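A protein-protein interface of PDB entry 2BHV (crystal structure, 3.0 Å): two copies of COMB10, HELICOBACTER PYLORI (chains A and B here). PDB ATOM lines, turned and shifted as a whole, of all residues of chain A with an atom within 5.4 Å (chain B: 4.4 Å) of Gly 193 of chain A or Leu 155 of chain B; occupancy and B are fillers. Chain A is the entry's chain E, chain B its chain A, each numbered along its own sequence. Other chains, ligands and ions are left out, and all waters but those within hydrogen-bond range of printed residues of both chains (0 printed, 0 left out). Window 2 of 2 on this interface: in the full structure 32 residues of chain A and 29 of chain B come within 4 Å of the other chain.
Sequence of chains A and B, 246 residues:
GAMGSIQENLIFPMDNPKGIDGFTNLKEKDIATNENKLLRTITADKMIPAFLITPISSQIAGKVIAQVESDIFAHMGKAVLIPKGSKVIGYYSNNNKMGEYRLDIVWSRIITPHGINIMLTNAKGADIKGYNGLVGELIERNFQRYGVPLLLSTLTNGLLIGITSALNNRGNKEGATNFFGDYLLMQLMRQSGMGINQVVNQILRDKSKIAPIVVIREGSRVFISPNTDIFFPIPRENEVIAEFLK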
ATOM      1  N   GLN A 191      33.244  -3.960 -12.939  1.00  0.00           N
ATOM      2  CA  GLN A 191      32.359  -3.529 -14.047  1.00  0.00           C
ATOM      3  C   GLN A 191      32.016  -4.539 -15.172  1.00  0.00           C
ATOM      4  O   GLN A 191      31.941  -4.176 -16.341  1.00  0.00           O
ATOM      5  CB  GLN A 191      32.831  -2.181 -14.630  1.00  0.00           C
ATOM      6  CG  GLN A 191      34.245  -2.150 -15.205  1.00  0.00           C
ATOM      7  CD  GLN A 191      34.959  -0.818 -14.958  1.00  0.00           C
ATOM      8  OE1 GLN A 191      35.196  -0.033 -15.887  1.00  0.00           O
ATOM      9  NE2 GLN A 191      35.307  -0.561 -13.701  1.00  0.00           N
ATOM     10  N   SER A 192      31.771  -5.794 -14.815  1.00  0.00           N
ATOM     11  CA  SER A 192      31.287  -6.760 -15.797  1.00  0.00           C
ATOM     12  C   SER A 192      29.884  -6.413 -16.229  1.00  0.00           C
ATOM     13  O   SER A 192      29.048  -6.099 -15.402  1.00  0.00           O
ATOM     14  CB  SER A 192      31.285  -8.163 -15.230  1.00  0.00           C
ATOM     15  OG  SER A 192      30.418  -8.959 -15.995  1.00  0.00           O
ATOM     16  N   GLY A 193      29.618  -6.482 -17.521  1.00  0.00           N
ATOM     17  CA  GLY A 193      28.289  -6.172 -18.025  1.00  0.00           C
ATOM     18  C   GLY A 193      28.193  -4.763 -18.556  1.00  0.00           C
ATOM     19  O   GLY A 193      27.363  -4.472 -19.392  1.00  0.00           O
ATOM     20  N   MET A 194      29.048  -3.881 -18.067  1.00  0.00           N
ATOM     21  CA  MET A 194      29.102  -2.502 -18.533  1.00  0.00           C
ATOM     22  C   MET A 194      29.371  -2.476 -20.052  1.00  0.00           C
ATOM     23  O   MET A 194      29.882  -3.432 -20.600  1.00  0.00           O
ATOM     24  CB  MET A 194      30.206  -1.797 -17.758  1.00  0.00           C
ATOM     25  CG  MET A 194      30.191  -0.302 -17.747  1.00  0.00           C
ATOM     26  SD  MET A 194      31.376   0.258 -16.501  1.00  0.00           S
ATOM     27  CE  MET A 194      31.934   1.836 -17.137  1.00  0.00           C
ATOM     28  N   GLY A 195      29.012  -1.396 -20.729  1.00  0.00           N
ATOM     29  CA  GLY A 195      29.104  -1.340 -22.187  1.00  0.00           C
ATOM     30  C   GLY A 195      30.436  -0.773 -22.609  1.00  0.00           C
ATOM     31  O   GLY A 195      30.996   0.046 -21.896  1.00  0.00           O
ATOM     32  N   ILE A 196      30.941  -1.191 -23.770  1.00  0.00           N
ATOM     33  CA  ILE A 196      32.302  -0.856 -24.173  1.00  0.00           C
ATOM     34  C   ILE A 196      32.606   0.617 -23.934  1.00  0.00           C
ATOM     35  O   ILE A 196      33.484   0.962 -23.138  1.00  0.00           O
ATOM     36  CB  ILE A 196      32.594  -1.206 -25.651  1.00  0.00           C
ATOM     37  CG1 ILE A 196      32.397  -2.684 -25.899  1.00  0.00           C
ATOM     38  CG2 ILE A 196      34.025  -0.865 -26.023  1.00  0.00           C
ATOM     39  CD1 ILE A 196      33.058  -3.159 -27.174  1.00  0.00           C
ATOM     40  N   MET B  47      22.541 -12.516 -22.655  1.00  0.00           N
ATOM     41  CA  MET B  47      23.940 -12.178 -22.771  1.00  0.00           C
ATOM     42  C   MET B  47      24.586 -13.270 -23.573  1.00  0.00           C
ATOM     43  O   MET B  47      24.781 -14.368 -23.064  1.00  0.00           O
ATOM     44  CB  MET B  47      24.591 -12.093 -21.392  1.00  0.00           C
ATOM     45  CG  MET B  47      23.964 -11.116 -20.438  1.00  0.00           C
ATOM     46  SD  MET B  47      24.473  -9.432 -20.778  1.00  0.00           S
ATOM     47  CE  MET B  47      23.052  -8.831 -21.658  1.00  0.00           C
ATOM     48  N   SER B 153      23.650  -4.649 -28.425  1.00  0.00           N
ATOM     49  CA  SER B 153      24.646  -3.923 -27.671  1.00  0.00           C
ATOM     50  C   SER B 153      25.861  -4.800 -27.505  1.00  0.00           C
ATOM     51  O   SER B 153      25.761  -6.024 -27.600  1.00  0.00           O
ATOM     52  CB  SER B 153      24.096  -3.552 -26.311  1.00  0.00           C
ATOM     53  OG  SER B 153      23.018  -2.649 -26.446  1.00  0.00           O
ATOM     54  N   THR B 154      27.012  -4.173 -27.248  1.00  0.00           N
ATOM     55  CA  THR B 154      28.251  -4.897 -27.004  1.00  0.00           C
ATOM     56  C   THR B 154      28.790  -4.524 -25.657  1.00  0.00           C
ATOM     57  O   THR B 154      29.218  -3.409 -25.455  1.00  0.00           O
ATOM     58  CB  THR B 154      29.285  -4.592 -28.077  1.00  0.00           C
ATOM     59  OG1 THR B 154      28.657  -4.693 -29.359  1.00  0.00           O
ATOM     60  CG2 THR B 154      30.432  -5.552 -27.997  1.00  0.00           C
ATOM     61  N   LEU B 155      28.759  -5.487 -24.740  1.00  0.00           N
ATOM     62  CA  LEU B 155      29.126  -5.282 -23.334  1.00  0.00           C
ATOM     63  C   LEU B 155      30.434  -5.972 -22.983  1.00  0.00           C
ATOM     64  O   LEU B 155      30.853  -6.889 -23.689  1.00  0.00           O
ATOM     65  CB  LEU B 155      28.011  -5.810 -22.443  1.00  0.00           C
ATOM     66  CG  LEU B 155      26.679  -5.054 -22.301  1.00  0.00           C
ATOM     67  CD1 LEU B 155      26.384  -4.023 -23.383  1.00  0.00           C
ATOM     68  CD2 LEU B 155      25.529  -6.030 -22.174  1.00  0.00           C
ATOM     69  N   THR B 156      31.071  -5.544 -21.891  1.00  0.00           N
ATOM     70  CA  THR B 156      32.346  -6.130 -21.469  1.00  0.00           C
ATOM     71  C   THR B 156      32.155  -7.486 -20.883  1.00  0.00           C
ATOM     72  O   THR B 156      31.229  -7.709 -20.075  1.00  0.00           O
ATOM     73  CB  THR B 156      32.987  -5.409 -20.313  1.00  0.00           C
ATOM     74  OG1 THR B 156      32.468  -4.090 -20.208  1.00  0.00           O
ATOM     75  CG2 THR B 156      34.484  -5.411 -20.482  1.00  0.00           C
ATOM     76  N   ASN B 157      33.067  -8.383 -21.244  1.00  0.00           N
ATOM     77  CA  ASN B 157      33.303  -9.552 -20.437  1.00  0.00           C
ATOM     78  C   ASN B 157      34.793  -9.701 -20.166  1.00  0.00           C
ATOM     79  O   ASN B 157      35.290 -10.802 -19.967  1.00  0.00           O
ATOM     80  CB  ASN B 157      32.732 -10.777 -21.114  1.00  0.00           C
ATOM     81  CG  ASN B 157      32.659 -11.967 -20.192  1.00  0.00           C
ATOM     82  OD1 ASN B 157      32.579 -11.832 -18.977  1.00  0.00           O
ATOM     83  ND2 ASN B 157      32.687 -13.145 -20.772  1.00  0.00           N
ATOM     84  N   VAL B 222      33.556 -10.518 -24.552  1.00  0.00           N
ATOM     85  CA  VAL B 222      32.448  -9.605 -24.768  1.00  0.00           C
ATOM     86  C   VAL B 222      31.077 -10.286 -24.542  1.00  0.00           C
ATOM     87  O   VAL B 222      30.955 -11.491 -24.724  1.00  0.00           O
ATOM     88  CB  VAL B 222      32.591  -9.023 -26.193  1.00  0.00           C
ATOM     89  CG1 VAL B 222      31.338  -9.209 -27.027  1.00  0.00           C
ATOM     90  CG2 VAL B 222      33.064  -7.577 -26.142  1.00  0.00           C
ATOM     91  N   PHE B 223      30.069  -9.525 -24.122  1.00  0.00           N
ATOM     92  CA  PHE B 223      28.684  -9.986 -24.208  1.00  0.00           C
ATOM     93  C   PHE B 223      27.995  -9.250 -25.336  1.00  0.00           C
ATOM     94  O   PHE B 223      27.990  -8.019 -25.366  1.00  0.00           O
ATOM     95  CB  PHE B 223      27.900  -9.723 -22.915  1.00  0.00           C
ATOM     96  CG  PHE B 223      28.344 -10.543 -21.766  1.00  0.00           C
ATOM     97  CD1 PHE B 223      28.140 -11.908 -21.756  1.00  0.00           C
ATOM     98  CD2 PHE B 223      28.963  -9.957 -20.683  1.00  0.00           C
ATOM     99  CE1 PHE B 223      28.557 -12.673 -20.694  1.00  0.00           C
ATOM    100  CE2 PHE B 223      29.386 -10.728 -19.614  1.00  0.00           C
ATOM    101  CZ  PHE B 223      29.186 -12.086 -19.624  1.00  0.00           C
ATOM    102  N   SER B 225      24.391  -8.427 -26.678  1.00  0.00           N
ATOM    103  CA  SER B 225      23.077  -8.380 -26.062  1.00  0.00           C
ATOM    104  C   SER B 225      22.017  -7.758 -26.976  1.00  0.00           C
ATOM    105  O   SER B 225      22.140  -6.614 -27.400  1.00  0.00           O
ATOM    106  CB  SER B 225      23.163  -7.607 -24.758  1.00  0.00           C
ATOM    107  OG  SER B 225      21.881  -7.472 -24.167  1.00  0.00           O
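Among the printed residues, pairs that only touch across the chains: Gly 193 of chain A with Leu 155 of chain B (3.0 Å), Met 194 of chain A with Leu 155 of chain B (3.4 Å), Gly 195 of chain A with Thr 154 of chain B (3.9 Å) and Gln 191 of chain A with Thr 156 of chain B (3.9 Å).
Of the 9 printed residues of chain B, 3 touch a printed residue of chain A.
Along chain A the printed residues that touch a printed residue of chain B span positions 191 to 196.
Among the printed residues, 7 pairs touch across the chains.
O of Phe 223 of chain B sits at hydrogen-bond distance from N of Leu 155 of chain B (2.7 Å).
The backbone carbonyl oxygen (O) of Thr 154 of chain B is in hydrogen-bond range of the backbone NH (N) of Ile 196 of chain A (3.3 Å).
The backbone carbonyl oxygen (O) of Thr 156 of chain B lies within hydrogen-bond range of the backbone NH (N) of Gly 193 of chain A (3.3 Å).
The backbone carbonyl oxygen (O) of Met 194 of chain A is in hydrogen-bond range of the side-chain hydroxyl (OG1) of Thr 156 of chain B, 2.7 Å away.
No position is printed for both chains.
Of the 7 pairs that touch across the chains among the printed residues, none has its exchanged pair printed and touching as well.
Printed residues of chain A within 4 Å of Leu 155 of chain B: Gly 193 (3.0 Å) and Met 194 (3.4 Å).
Of the printed residues of chain B, Ile 196 of chain A touches Thr 154.
Printed residues of chain B within 4 Å of Gly 195 of chain A: Thr 154.
Of the printed residues of chain B, Met 194 of chain A touches Leu 155 and Thr 156.
Ser 153 of chain B touches none of the printed residues of chain A.
Phe 223 of chain B touches none of the printed residues of chain A.
The nearest printed residue of chain B that does not touch Gly 193 of chain A is Phe 223 of chain B (4.7 Å).
The nearest printed residue of chain A that does not touch Thr 156 of chain B is Ser 192 of chain A (4.3 Å).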
